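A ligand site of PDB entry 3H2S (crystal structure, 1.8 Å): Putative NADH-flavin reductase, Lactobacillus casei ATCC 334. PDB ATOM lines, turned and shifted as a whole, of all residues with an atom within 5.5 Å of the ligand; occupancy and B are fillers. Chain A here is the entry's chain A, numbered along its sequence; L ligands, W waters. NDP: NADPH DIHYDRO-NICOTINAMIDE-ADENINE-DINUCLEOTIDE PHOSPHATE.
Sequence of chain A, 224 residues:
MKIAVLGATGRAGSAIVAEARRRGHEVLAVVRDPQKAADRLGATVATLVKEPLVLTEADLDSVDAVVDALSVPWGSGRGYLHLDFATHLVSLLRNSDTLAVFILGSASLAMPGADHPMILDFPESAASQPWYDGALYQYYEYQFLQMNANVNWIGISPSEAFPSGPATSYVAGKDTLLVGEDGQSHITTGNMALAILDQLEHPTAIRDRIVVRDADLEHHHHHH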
ATOM      1  N   GLY A   7     -10.387  -5.955  -4.720  1.00  0.00           N
ATOM      2  CA  GLY A   7     -10.499  -6.763  -5.941  1.00  0.00           C
ATOM      3  C   GLY A   7     -10.602  -5.865  -7.170  1.00  0.00           C
ATOM      4  O   GLY A   7     -11.225  -6.229  -8.160  1.00  0.00           O
ATOM      5  N   ALA A   8      -9.867  -4.754  -7.141  1.00  0.00           N
ATOM      6  CA  ALA A   8      -9.859  -3.767  -8.232  1.00  0.00           C
ATOM      7  C   ALA A   8      -9.310  -4.306  -9.565  1.00  0.00           C
ATOM      8  O   ALA A   8      -9.694  -3.819 -10.626  1.00  0.00           O
ATOM      9  CB  ALA A   8      -9.063  -2.515  -7.800  1.00  0.00           C
ATOM     10  N   THR A   9      -8.473  -5.334  -9.505  1.00  0.00           N
ATOM     11  CA  THR A   9      -7.901  -5.939 -10.723  1.00  0.00           C
ATOM     12  C   THR A   9      -8.794  -7.020 -11.341  1.00  0.00           C
ATOM     13  O   THR A   9      -8.533  -7.476 -12.475  1.00  0.00           O
ATOM     14  CB  THR A   9      -6.499  -6.537 -10.460  1.00  0.00           C
ATOM     15  OG1 THR A   9      -6.577  -7.485  -9.385  1.00  0.00           O
ATOM     16  CG2 THR A   9      -5.526  -5.422 -10.101  1.00  0.00           C
ATOM     17  N   GLY A  10      -9.878  -7.349 -10.650  1.00  0.00           N
ATOM     18  CA  GLY A  10     -10.802  -8.390 -11.124  1.00  0.00           C
ATOM     19  C   GLY A  10     -11.699  -7.912 -12.253  1.00  0.00           C
ATOM     20  O   GLY A  10     -11.616  -6.757 -12.688  1.00  0.00           O
ATOM     21  N   ARG A  11     -12.609  -8.778 -12.682  1.00  0.00           N
ATOM     22  CA  ARG A  11     -13.521  -8.449 -13.783  1.00  0.00           C
ATOM     23  C   ARG A  11     -14.495  -7.356 -13.355  1.00  0.00           C
ATOM     24  O   ARG A  11     -14.576  -6.314 -14.009  1.00  0.00           O
ATOM     25  CB  ARG A  11     -14.272  -9.703 -14.235  1.00  0.00           C
ATOM     26  CG  ARG A  11     -13.325 -10.860 -14.679  1.00  0.00           C
ATOM     27  CD  ARG A  11     -14.056 -12.190 -14.787  1.00  0.00           C
ATOM     28  NE  ARG A  11     -15.109 -12.133 -15.789  1.00  0.00           N
ATOM     29  CZ  ARG A  11     -16.415 -12.127 -15.511  1.00  0.00           C
ATOM     30  NH1 ARG A  11     -16.840 -12.204 -14.250  1.00  0.00           N
ATOM     31  NH2 ARG A  11     -17.289 -12.085 -16.496  1.00  0.00           N
ATOM     32  N   ALA A  12     -15.222  -7.584 -12.266  1.00  0.00           N
ATOM     33  CA  ALA A  12     -16.138  -6.566 -11.703  1.00  0.00           C
ATOM     34  C   ALA A  12     -15.352  -5.343 -11.224  1.00  0.00           C
ATOM     35  O   ALA A  12     -15.700  -4.200 -11.547  1.00  0.00           O
ATOM     36  CB  ALA A  12     -16.962  -7.142 -10.563  1.00  0.00           C
ATOM     37  N   GLY A  13     -14.255  -5.595 -10.519  1.00  0.00           N
ATOM     38  CA  GLY A  13     -13.444  -4.523  -9.931  1.00  0.00           C
ATOM     39  C   GLY A  13     -12.886  -3.516 -10.914  1.00  0.00           C
ATOM     40  O   GLY A  13     -12.952  -2.306 -10.691  1.00  0.00           O
ATOM     41  N   ARG A  32      -3.009  -7.026  -5.092  1.00  0.00           N
ATOM     42  CA  ARG A  32      -1.860  -7.834  -4.724  1.00  0.00           C
ATOM     43  C   ARG A  32      -0.861  -7.901  -5.869  1.00  0.00           C
ATOM     44  O   ARG A  32       0.294  -8.259  -5.665  1.00  0.00           O
ATOM     45  CB  ARG A  32      -2.302  -9.222  -4.296  1.00  0.00           C
ATOM     46  CG  ARG A  32      -3.149  -9.935  -5.325  1.00  0.00           C
ATOM     47  CD  ARG A  32      -3.497 -11.343  -4.849  1.00  0.00           C
ATOM     48  NE  ARG A  32      -4.302 -12.030  -5.846  1.00  0.00           N
ATOM     49  CZ  ARG A  32      -4.766 -13.261  -5.706  1.00  0.00           C
ATOM     50  NH1 ARG A  32      -4.453 -13.975  -4.623  1.00  0.00           N
ATOM     51  NH2 ARG A  32      -5.492 -13.799  -6.680  1.00  0.00           N
ATOM     52  N   ASP A  33      -1.287  -7.485  -7.056  1.00  0.00           N
ATOM     53  CA  ASP A  33      -0.518  -7.672  -8.281  1.00  0.00           C
ATOM     54  C   ASP A  33      -0.321  -6.328  -8.982  1.00  0.00           C
ATOM     55  O   ASP A  33      -1.143  -5.920  -9.816  1.00  0.00           O
ATOM     56  CB  ASP A  33      -1.266  -8.635  -9.210  1.00  0.00           C
ATOM     57  CG  ASP A  33      -0.474  -8.982 -10.468  1.00  0.00           C
ATOM     58  OD1 ASP A  33       0.369  -8.158 -10.885  1.00  0.00           O
ATOM     59  OD2 ASP A  33      -0.742 -10.062 -11.039  1.00  0.00           O
ATOM     60  N   LYS A  36      -0.581  -6.374 -12.828  1.00  0.00           N
ATOM     61  CA  LYS A  36      -1.992  -6.462 -13.209  1.00  0.00           C
ATOM     62  C   LYS A  36      -2.648  -5.095 -13.070  1.00  0.00           C
ATOM     63  O   LYS A  36      -3.457  -4.693 -13.905  1.00  0.00           O
ATOM     64  CB  LYS A  36      -2.716  -7.503 -12.359  1.00  0.00           C
ATOM     65  CG  LYS A  36      -3.728  -8.360 -13.128  1.00  0.00           C
ATOM     66  CD  LYS A  36      -4.372  -9.416 -12.229  1.00  0.00           C
ATOM     67  CE  LYS A  36      -3.507 -10.674 -12.139  1.00  0.00           C
ATOM     68  NZ  LYS A  36      -3.446 -11.215 -10.740  1.00  0.00           N
ATOM     69  N   ARG A  40      -4.322  -3.203 -16.173  1.00  0.00           N
ATOM     70  CA  ARG A  40      -5.791  -3.225 -16.227  1.00  0.00           C
ATOM     71  C   ARG A  40      -6.435  -1.909 -15.812  1.00  0.00           C
ATOM     72  O   ARG A  40      -7.617  -1.665 -16.076  1.00  0.00           O
ATOM     73  CB  ARG A  40      -6.358  -4.384 -15.408  1.00  0.00           C
ATOM     74  CG  ARG A  40      -6.020  -5.735 -15.975  1.00  0.00           C
ATOM     75  CD  ARG A  40      -6.505  -6.887 -15.106  1.00  0.00           C
ATOM     76  NE  ARG A  40      -6.162  -8.167 -15.717  1.00  0.00           N
ATOM     77  CZ  ARG A  40      -6.439  -9.356 -15.183  1.00  0.00           C
ATOM     78  NH1 ARG A  40      -7.110  -9.458 -14.044  1.00  0.00           N
ATOM     79  NH2 ARG A  40      -6.047 -10.464 -15.810  1.00  0.00           N
ATOM     80  N   PRO A  52      -6.182  -7.987   1.700  1.00  0.00           N
ATOM     81  CA  PRO A  52      -7.418  -7.399   2.217  1.00  0.00           C
ATOM     82  C   PRO A  52      -7.628  -7.678   3.701  1.00  0.00           C
ATOM     83  O   PRO A  52      -8.100  -6.805   4.409  1.00  0.00           O
ATOM     84  CB  PRO A  52      -8.502  -8.073   1.374  1.00  0.00           C
ATOM     85  CG  PRO A  52      -7.823  -8.377   0.080  1.00  0.00           C
ATOM     86  CD  PRO A  52      -6.376  -8.694   0.427  1.00  0.00           C
ATOM     87  N   ASP A  68     -16.511  -3.999  -2.263  1.00  0.00           N
ATOM     88  CA  ASP A  68     -15.953  -5.352  -2.159  1.00  0.00           C
ATOM     89  C   ASP A  68     -16.222  -6.141  -3.458  1.00  0.00           C
ATOM     90  O   ASP A  68     -17.330  -6.641  -3.665  1.00  0.00           O
ATOM     91  CB  ASP A  68     -16.501  -6.084  -0.923  1.00  0.00           C
ATOM     92  CG  ASP A  68     -15.989  -7.512  -0.785  1.00  0.00           C
ATOM     93  OD1 ASP A  68     -15.359  -8.040  -1.726  1.00  0.00           O
ATOM     94  OD2 ASP A  68     -16.240  -8.140   0.288  1.00  0.00           O
ATOM     95  N   ALA A  69     -15.244  -6.173  -4.360  1.00  0.00           N
ATOM     96  CA  ALA A  69     -15.362  -6.939  -5.587  1.00  0.00           C
ATOM     97  C   ALA A  69     -14.403  -8.128  -5.602  1.00  0.00           C
ATOM     98  O   ALA A  69     -13.969  -8.563  -6.665  1.00  0.00           O
ATOM     99  CB  ALA A  69     -15.097  -6.042  -6.818  1.00  0.00           C
ATOM    100  N   LEU A  70     -14.035  -8.611  -4.421  1.00  0.00           N
ATOM    101  CA  LEU A  70     -13.158  -9.768  -4.312  1.00  0.00           C
ATOM    102  C   LEU A  70     -13.914 -11.046  -4.636  1.00  0.00           C
ATOM    103  O   LEU A  70     -15.129 -11.130  -4.395  1.00  0.00           O
ATOM    104  CB  LEU A  70     -12.584  -9.873  -2.879  1.00  0.00           C
ATOM    105  CG  LEU A  70     -11.633  -8.763  -2.450  1.00  0.00           C
ATOM    106  CD1 LEU A  70     -11.609  -8.636  -0.914  1.00  0.00           C
ATOM    107  CD2 LEU A  70     -10.228  -8.964  -3.016  1.00  0.00           C
ATOM    108  N   SER A  71     -13.189 -12.051  -5.126  1.00  0.00           N
ATOM    109  CA  SER A  71     -13.785 -13.359  -5.353  1.00  0.00           C
ATOM    110  C   SER A  71     -12.833 -14.504  -5.033  1.00  0.00           C
ATOM    111  O   SER A  71     -11.675 -14.271  -4.638  1.00  0.00           O
ATOM    112  CB  SER A  71     -14.278 -13.480  -6.785  1.00  0.00           C
ATOM    113  OG  SER A  71     -15.288 -14.472  -6.863  1.00  0.00           O
ATOM    114  N   VAL A  72     -13.318 -15.716  -5.212  1.00  0.00           N
ATOM    115  CA  VAL A  72     -12.558 -16.915  -4.925  1.00  0.00           C
ATOM    116  C   VAL A  72     -12.748 -17.879  -6.089  1.00  0.00           C
ATOM    117  O   VAL A  72     -13.894 -18.197  -6.451  1.00  0.00           O
ATOM    118  CB  VAL A  72     -13.067 -17.612  -3.656  1.00  0.00           C
ATOM    119  CG1 VAL A  72     -12.244 -18.862  -3.355  1.00  0.00           C
ATOM    120  CG2 VAL A  72     -13.038 -16.652  -2.462  1.00  0.00           C
ATOM    121  N   PRO A  73     -11.639 -18.420  -6.622  1.00  0.00           N
ATOM    122  CA  PRO A  73     -11.766 -19.385  -7.716  1.00  0.00           C
ATOM    123  C   PRO A  73     -12.521 -20.641  -7.286  1.00  0.00           C
ATOM    124  O   PRO A  73     -12.356 -21.126  -6.153  1.00  0.00           O
ATOM    125  CB  PRO A  73     -10.298 -19.733  -8.035  1.00  0.00           C
ATOM    126  CG  PRO A  73      -9.484 -18.618  -7.424  1.00  0.00           C
ATOM    127  CD  PRO A  73     -10.247 -18.234  -6.193  1.00  0.00           C
ATOM    128  N   LEU A  81     -13.237 -17.285   2.182  1.00  0.00           N
ATOM    129  CA  LEU A  81     -12.756 -15.904   2.015  1.00  0.00           C
ATOM    130  C   LEU A  81     -13.846 -14.900   1.674  1.00  0.00           C
ATOM    131  O   LEU A  81     -13.748 -13.732   2.042  1.00  0.00           O
ATOM    132  CB  LEU A  81     -11.629 -15.843   0.990  1.00  0.00           C
ATOM    133  CG  LEU A  81     -10.292 -16.477   1.371  1.00  0.00           C
ATOM    134  CD1 LEU A  81      -9.327 -16.404   0.197  1.00  0.00           C
ATOM    135  CD2 LEU A  81      -9.700 -15.789   2.599  1.00  0.00           C
ATOM    136  N   HIS A  82     -14.870 -15.331   0.941  1.00  0.00           N
ATOM    137  CA  HIS A  82     -16.013 -14.467   0.698  1.00  0.00           C
ATOM    138  C   HIS A  82     -16.532 -13.894   2.024  1.00  0.00           C
ATOM    139  O   HIS A  82     -16.835 -12.704   2.125  1.00  0.00           O
ATOM    140  CB  HIS A  82     -17.129 -15.231  -0.002  1.00  0.00           C
ATOM    141  CG  HIS A  82     -16.924 -15.367  -1.470  1.00  0.00           C
ATOM    142  ND1 HIS A  82     -16.715 -16.583  -2.085  1.00  0.00           N
ATOM    143  CD2 HIS A  82     -16.906 -14.440  -2.456  1.00  0.00           C
ATOM    144  CE1 HIS A  82     -16.672 -16.410  -3.395  1.00  0.00           C
ATOM    145  NE2 HIS A  82     -16.760 -15.113  -3.647  1.00  0.00           N
ATOM    146  N   PHE A  85     -13.392 -11.805   4.129  1.00  0.00           N
ATOM    147  CA  PHE A  85     -13.129 -10.451   3.629  1.00  0.00           C
ATOM    148  C   PHE A  85     -14.239  -9.507   4.126  1.00  0.00           C
ATOM    149  O   PHE A  85     -13.976  -8.344   4.453  1.00  0.00           O
ATOM    150  CB  PHE A  85     -13.122 -10.415   2.106  1.00  0.00           C
ATOM    151  CG  PHE A  85     -12.025 -11.234   1.469  1.00  0.00           C
ATOM    152  CD1 PHE A  85     -10.707 -11.134   1.912  1.00  0.00           C
ATOM    153  CD2 PHE A  85     -12.261 -11.900   0.281  1.00  0.00           C
ATOM    154  CE1 PHE A  85      -9.671 -11.724   1.225  1.00  0.00           C
ATOM    155  CE2 PHE A  85     -11.204 -12.513  -0.419  1.00  0.00           C
ATOM    156  CZ  PHE A  85      -9.928 -12.446   0.082  1.00  0.00           C
ATOM    157  N   ILE A 103     -20.663  -7.035  -3.469  1.00  0.00           N
ATOM    158  CA  ILE A 103     -21.213  -7.839  -4.537  1.00  0.00           C
ATOM    159  C   ILE A 103     -21.431  -9.254  -3.992  1.00  0.00           C
ATOM    160  O   ILE A 103     -20.498  -9.909  -3.530  1.00  0.00           O
ATOM    161  CB  ILE A 103     -20.294  -7.942  -5.775  1.00  0.00           C
ATOM    162  CG1 ILE A 103     -19.974  -6.537  -6.351  1.00  0.00           C
ATOM    163  CG2 ILE A 103     -20.960  -8.807  -6.817  1.00  0.00           C
ATOM    164  CD1 ILE A 103     -19.077  -6.585  -7.574  1.00  0.00           C
ATOM    165  N   LEU A 104     -22.665  -9.717  -4.094  1.00  0.00           N
ATOM    166  CA  LEU A 104     -23.047 -10.996  -3.517  1.00  0.00           C
ATOM    167  C   LEU A 104     -23.247 -12.022  -4.636  1.00  0.00           C
ATOM    168  O   LEU A 104     -22.735 -11.848  -5.738  1.00  0.00           O
ATOM    169  CB  LEU A 104     -24.326 -10.833  -2.673  1.00  0.00           C
ATOM    170  CG  LEU A 104     -24.163  -9.884  -1.471  1.00  0.00           C
ATOM    171  CD1 LEU A 104     -25.506  -9.600  -0.817  1.00  0.00           C
ATOM    172  CD2 LEU A 104     -23.151 -10.425  -0.458  1.00  0.00           C
ATOM    173  N   GLY A 105     -23.871 -13.140  -4.305  1.00  0.00           N
ATOM    174  CA  GLY A 105     -24.080 -14.203  -5.286  1.00  0.00           C
ATOM    175  C   GLY A 105     -25.532 -14.295  -5.697  1.00  0.00           C
ATOM    176  O   GLY A 105     -26.420 -13.751  -5.034  1.00  0.00           O
ATOM    177  N   SER A 106     -25.774 -15.061  -6.753  1.00  0.00           N
ATOM    178  CA  SER A 106     -27.108 -15.303  -7.258  1.00  0.00           C
ATOM    179  C   SER A 106     -27.849 -16.331  -6.387  1.00  0.00           C
ATOM    180  O   SER A 106     -29.074 -16.348  -6.341  1.00  0.00           O
ATOM    181  CB  SER A 106     -26.997 -15.794  -8.705  1.00  0.00           C
ATOM    182  OG  SER A 106     -28.018 -15.243  -9.506  1.00  0.00           O
ATOM    183  N   ALA A 107     -27.106 -17.172  -5.689  1.00  0.00           N
ATOM    184  CA  ALA A 107     -27.704 -18.302  -4.968  1.00  0.00           C
ATOM    185  C   ALA A 107     -28.488 -17.895  -3.725  1.00  0.00           C
ATOM    186  O   ALA A 107     -29.263 -18.682  -3.174  1.00  0.00           O
ATOM    187  CB  ALA A 107     -26.644 -19.339  -4.629  1.00  0.00           C
ATOM    188  N   GLN A 138     -20.982 -17.086   0.225  1.00  0.00           N
ATOM    189  CA  GLN A 138     -21.617 -15.817  -0.156  1.00  0.00           C
ATOM    190  C   GLN A 138     -23.032 -15.692   0.364  1.00  0.00           C
ATOM    191  O   GLN A 138     -23.510 -14.588   0.630  1.00  0.00           O
ATOM    192  CB  GLN A 138     -21.583 -15.608  -1.665  1.00  0.00           C
ATOM    193  CG  GLN A 138     -20.223 -15.226  -2.162  1.00  0.00           C
ATOM    194  CD  GLN A 138     -20.278 -14.190  -3.249  1.00  0.00           C
ATOM    195  OE1 GLN A 138     -20.523 -14.515  -4.409  1.00  0.00           O
ATOM    196  NE2 GLN A 138     -19.982 -12.950  -2.905  1.00  0.00           N
ATOM    197  N   PRO A 158     -25.656 -10.178  -8.532  1.00  0.00           N
ATOM    198  CA  PRO A 158     -25.772 -10.296  -9.966  1.00  0.00           C
ATOM    199  C   PRO A 158     -26.973 -11.168 -10.334  1.00  0.00           C
ATOM    200  O   PRO A 158     -27.435 -11.948  -9.513  1.00  0.00           O
ATOM    201  CB  PRO A 158     -24.456 -10.979 -10.392  1.00  0.00           C
ATOM    202  CG  PRO A 158     -23.597 -11.083  -9.141  1.00  0.00           C
ATOM    203  CD  PRO A 158     -24.541 -10.993  -7.994  1.00  0.00           C
ATOM    204  N   SER A 159     -27.369 -11.113 -11.591  1.00  0.00           N
ATOM    205  CA  SER A 159     -28.184 -12.176 -12.178  1.00  0.00           C
ATOM    206  C   SER A 159     -27.353 -13.441 -12.289  1.00  0.00           C
ATOM    207  O   SER A 159     -26.144 -13.430 -12.084  1.00  0.00           O
ATOM    208  CB  SER A 159     -28.656 -11.740 -13.564  1.00  0.00           C
ATOM    209  OG  SER A 159     -29.351 -10.514 -13.477  1.00  0.00           O
ATOM    210  N   GLU A 160     -27.975 -14.508 -12.796  1.00  0.00           N
ATOM    211  CA  GLU A 160     -27.335 -15.811 -12.869  1.00  0.00           C
ATOM    212  C   GLU A 160     -26.036 -15.763 -13.675  1.00  0.00           C
ATOM    213  O   GLU A 160     -25.062 -16.457 -13.337  1.00  0.00           O
ATOM    214  CB  GLU A 160     -28.306 -16.804 -13.499  1.00  0.00           C
ATOM    215  CG  GLU A 160     -27.651 -17.908 -14.308  1.00  0.00           C
ATOM    216  CD  GLU A 160     -28.392 -19.229 -14.194  1.00  0.00           C
ATOM    217  OE1 GLU A 160     -29.308 -19.319 -13.343  1.00  0.00           O
ATOM    218  OE2 GLU A 160     -28.051 -20.173 -14.947  1.00  0.00           O
ATOM    219  N   ALA A 161     -26.007 -14.936 -14.720  1.00  0.00           N
ATOM    220  CA  ALA A 161     -24.816 -14.831 -15.561  1.00  0.00           C
ATOM    221  C   ALA A 161     -24.154 -13.470 -15.390  1.00  0.00           C
ATOM    222  O   ALA A 161     -24.817 -12.443 -15.490  1.00  0.00           O
ATOM    223  CB  ALA A 161     -25.158 -15.082 -17.035  1.00  0.00           C
ATOM    224  N   PHE A 162     -22.833 -13.468 -15.186  1.00  0.00           N
ATOM    225  CA  PHE A 162     -22.094 -12.222 -14.935  1.00  0.00           C
ATOM    226  C   PHE A 162     -20.939 -12.042 -15.950  1.00  0.00           C
ATOM    227  O   PHE A 162     -19.762 -11.963 -15.569  1.00  0.00           O
ATOM    228  CB  PHE A 162     -21.575 -12.244 -13.485  1.00  0.00           C
ATOM    229  CG  PHE A 162     -21.095 -10.911 -12.974  1.00  0.00           C
ATOM    230  CD1 PHE A 162     -21.359  -9.734 -13.667  1.00  0.00           C
ATOM    231  CD2 PHE A 162     -20.390 -10.845 -11.778  1.00  0.00           C
ATOM    232  CE1 PHE A 162     -20.951  -8.517 -13.155  1.00  0.00           C
ATOM    233  CE2 PHE A 162     -19.968  -9.632 -11.267  1.00  0.00           C
ATOM    234  CZ  PHE A 162     -20.228  -8.464 -11.971  1.00  0.00           C
HETATM  235  PA  NDP L   1     -12.484 -11.988 -10.303  1.00  0.00           P
HETATM  236  O1A NDP L   1     -12.247 -13.530 -10.283  1.00  0.00           O
HETATM  237  O2A NDP L   1     -12.297 -11.270 -11.588  1.00  0.00           O
HETATM  238  O5B NDP L   1     -11.242 -11.641  -9.197  1.00  0.00           O
HETATM  239  C5B NDP L   1     -11.785 -10.805  -8.140  1.00  0.00           C
HETATM  240  C4B NDP L   1     -10.619 -10.116  -7.336  1.00  0.00           C
HETATM  241  O4B NDP L   1     -10.276 -10.958  -6.254  1.00  0.00           O
HETATM  242  C3B NDP L   1      -9.304  -9.972  -8.174  1.00  0.00           C
HETATM  243  O3B NDP L   1      -8.945  -8.628  -8.113  1.00  0.00           O
HETATM  244  C2B NDP L   1      -8.287 -10.884  -7.363  1.00  0.00           C
HETATM  245  O2B NDP L   1      -6.962 -10.503  -7.379  1.00  0.00           O
HETATM  246  C1B NDP L   1      -8.924 -10.746  -5.953  1.00  0.00           C
HETATM  247  N9A NDP L   1      -8.509 -11.854  -5.085  1.00  0.00           N
HETATM  248  C8A NDP L   1      -8.880 -13.213  -5.287  1.00  0.00           C
HETATM  249  N7A NDP L   1      -8.411 -14.034  -4.345  1.00  0.00           N
HETATM  250  C5A NDP L   1      -7.716 -13.176  -3.464  1.00  0.00           C
HETATM  251  C6A NDP L   1      -7.034 -13.477  -2.269  1.00  0.00           C
HETATM  252  N6A NDP L   1      -6.949 -14.777  -1.877  1.00  0.00           N
HETATM  253  N1A NDP L   1      -6.213 -12.505  -1.730  1.00  0.00           N
HETATM  254  C2A NDP L   1      -6.382 -11.233  -2.195  1.00  0.00           C
HETATM  255  N3A NDP L   1      -7.172 -10.786  -3.216  1.00  0.00           N
HETATM  256  C4A NDP L   1      -7.779 -11.821  -3.892  1.00  0.00           C
HETATM  257  O3  NDP L   1     -14.009 -11.985  -9.902  1.00  0.00           O
HETATM  258  PN  NDP L   1     -15.421 -11.421 -10.449  1.00  0.00           P
HETATM  259  O1N NDP L   1     -15.236  -9.936 -10.827  1.00  0.00           O
HETATM  260  O2N NDP L   1     -15.722 -12.298 -11.625  1.00  0.00           O
HETATM  261  O5D NDP L   1     -16.562 -11.457  -9.282  1.00  0.00           O
HETATM  262  C5D NDP L   1     -16.809 -10.354  -8.415  1.00  0.00           C
HETATM  263  C4D NDP L   1     -17.981 -10.750  -7.489  1.00  0.00           C
HETATM  264  O4D NDP L   1     -19.000 -11.212  -8.345  1.00  0.00           O
HETATM  265  C3D NDP L   1     -17.715 -11.849  -6.428  1.00  0.00           C
HETATM  266  O3D NDP L   1     -18.458 -11.591  -5.278  1.00  0.00           O
HETATM  267  C2D NDP L   1     -18.203 -13.120  -7.205  1.00  0.00           C
HETATM  268  O2D NDP L   1     -18.654 -14.117  -6.322  1.00  0.00           O
HETATM  269  C1D NDP L   1     -19.446 -12.482  -7.917  1.00  0.00           C
HETATM  270  N1N NDP L   1     -19.965 -13.362  -8.971  1.00  0.00           N
HETATM  271  C2N NDP L   1     -21.292 -13.914  -8.739  1.00  0.00           C
HETATM  272  C3N NDP L   1     -21.705 -15.006  -9.722  1.00  0.00           C
HETATM  273  C7N NDP L   1     -23.218 -15.135  -9.744  1.00  0.00           C
HETATM  274  O7N NDP L   1     -23.843 -15.080  -8.693  1.00  0.00           O
HETATM  275  N7N NDP L   1     -23.842 -15.483 -10.924  1.00  0.00           N
HETATM  276  C4N NDP L   1     -21.069 -15.039 -11.103  1.00  0.00           C
HETATM  277  C5N NDP L   1     -19.603 -14.687 -11.122  1.00  0.00           C
HETATM  278  C6N NDP L   1     -19.084 -13.754 -10.053  1.00  0.00           C
HETATM  279  P2B NDP L   1      -6.016 -10.829  -8.666  1.00  0.00           P
HETATM  280  O1X NDP L   1      -6.459  -9.921  -9.861  1.00  0.00           O
HETATM  281  O2X NDP L   1      -4.589 -10.299  -8.308  1.00  0.00           O
HETATM  282  O3X NDP L   1      -6.054 -12.275  -9.048  1.00  0.00           O
HETATM  283  O   HOH W   1     -17.357 -16.176  -8.851  1.00  0.00           O
HETATM  284  O   HOH W   2     -12.509 -15.916  -9.117  1.00  0.00           O
HETATM  285  O   HOH W   3      -6.655 -13.998 -10.765  1.00  0.00           O
HETATM  286  O   HOH W   4     -17.271  -9.433  -4.572  1.00  0.00           O
HETATM  287  O   HOH W   5      -4.313  -7.783  -8.018  1.00  0.00           O
HETATM  288  O   HOH W   6      -7.152 -16.132  -6.847  1.00  0.00           O
HETATM  289  O   HOH W   7      -4.446 -11.944   0.645  1.00  0.00           O
HETATM  290  O   HOH W   8     -13.612  -8.156  -9.443  1.00  0.00           O
HETATM  291  O   HOH W   9      -7.369  -6.168  -6.802  1.00  0.00           O
HETATM  292  O   HOH W  10      -6.844  -8.381  -3.528  1.00  0.00           O
HETATM  293  O   HOH W  11     -10.041 -11.414 -12.917  1.00  0.00           O
HETATM  294  O   HOH W  12      -8.849 -14.365  -8.867  1.00  0.00           O
HETATM  295  O   HOH W  13     -21.827 -15.809 -14.064  1.00  0.00           O
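The guanidinium group of Arg 32 lies within salt-bridge range of an oxygen (O3X) of the ligand (2.9 Å). An oxygen (O3B) of the ligand is in hydrogen-bond range of the backbone NH of Gly 10, 3.0 Å away. NZ of Lys 36 is in salt-bridge range of O2X of the ligand (2.8 Å). The side-chain amide oxygen (OE1) of Gln 138 lies within hydrogen-bond range of an oxygen (O2D) of the ligand, at 2.7 Å. The backbone carbonyl oxygen (O) of Glu 160 is in hydrogen-bond range of a nitrogen (N7N) of the ligand. OG of Ser 71 sits close to O2D of the ligand (3.4 Å). The backbone NH of Ala 12 sits at hydrogen-bond distance from an oxygen (O1N) of the ligand. The backbone carbonyl oxygen (O) of Ile 103 is in hydrogen-bond range of an oxygen (O3D) of the ligand, at 3.2 Å. An oxygen (O3D) of the ligand lies close to the backbone carbonyl oxygen (O) of Leu 70 (3.5 Å). O3B of the ligand lies close to O of Gly 7 (3.3 Å). O of Ser 159 lies within hydrogen-bond range of N7N of the ligand (3.3 Å). An oxygen (O2A) of the ligand lies within hydrogen-bond range of the backbone NH of Arg 11 (2.7 Å). O2N of the ligand lies within salt-bridge range of NH1 of Arg 11 (2.9 Å). The backbone NH (N) of Ser 71 lies within hydrogen-bond range of an oxygen (O4B) of the ligand (3.3 Å). A ring nitrogen (NE2) of His 82 is in hydrogen-bond range of an oxygen (O2D) of the ligand (3.4 Å). The backbone NH (N) of Ser 106 sits at hydrogen-bond distance from an oxygen (O7N) of the ligand (2.7 Å). An oxygen (O1X) of the ligand lies within hydrogen-bond range of the side-chain hydroxyl (OG1) of Thr 9, at 2.5 Å.
The backbone NH of Glu 160 lies within hydrogen-bond range of the side-chain hydroxyl of Ser 106, at 3.4 Å. The side-chain hydroxyl (OG) of Ser 106 is in hydrogen-bond range of the backbone carbonyl oxygen (O) of Pro 158, at 3.3 Å. NE2 of Gln 138 is in hydrogen-bond range of O of Ile 103. OD2 of Asp 33 is in salt-bridge range of NZ of Lys 36 (3.0 Å). The guanidinium group of Arg 11 lies within hydrogen-bond range of the backbone carbonyl oxygen of Phe 162, 2.6 Å away. N of Leu 70 is in hydrogen-bond range of OD1 of Asp 68, at 3.1 Å. The backbone carbonyl oxygen (O) of Thr 9 is in hydrogen-bond range of the guanidinium group (NH1) of Arg 40, at 2.9 Å. O of Asp 68 sits at hydrogen-bond distance from N of Ile 103, at 3.4 Å.
Residues that only touch the ligand: Asp 33, Pro 52, Ala 69, Leu 81, Phe 85, Leu 104, Gly 105, Pro 158 and Phe 162. Hydrophobic or aromatic side chains that line the ligand: Ala 12, Pro 52, Leu 70, Leu 81, Phe 85, Ile 103, Pro 158 and Phe 162. 24 residues have an atom within 4 Å of the ligand: Gly 7, Thr 9, Gly 10, Arg 11, Ala 12, Arg 32, Asp 33, Lys 36, Pro 52, Ala 69, Leu 70, Ser 71, Leu 81, His 82, Phe 85, Ile 103, Leu 104, Gly 105, Ser 106, Gln 138, Pro 158, Ser 159, Glu 160 and Phe 162. The nearest printed residue that does not touch the ligand is Ala 8 (4.1 Å).
Water W5 lies within hydrogen-bond range of an oxygen (O2X) of the ligand (2.5 Å), the side-chain hydroxyl of Thr 9 (2.7 Å), the backbone NH of Asp 33 (3.2 Å) and the backbone NH of Arg 32 (3.3 Å). Water W9 lies within hydrogen-bond range of the backbone NH of Ala 8, the side-chain hydroxyl of Thr 9 and an oxygen (O3B) of the ligand. Water W6 bridges the guanidinium group (NH2) of Arg 32 (2.9 Å) and a nitrogen (N7A) of the ligand (3.5 Å).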
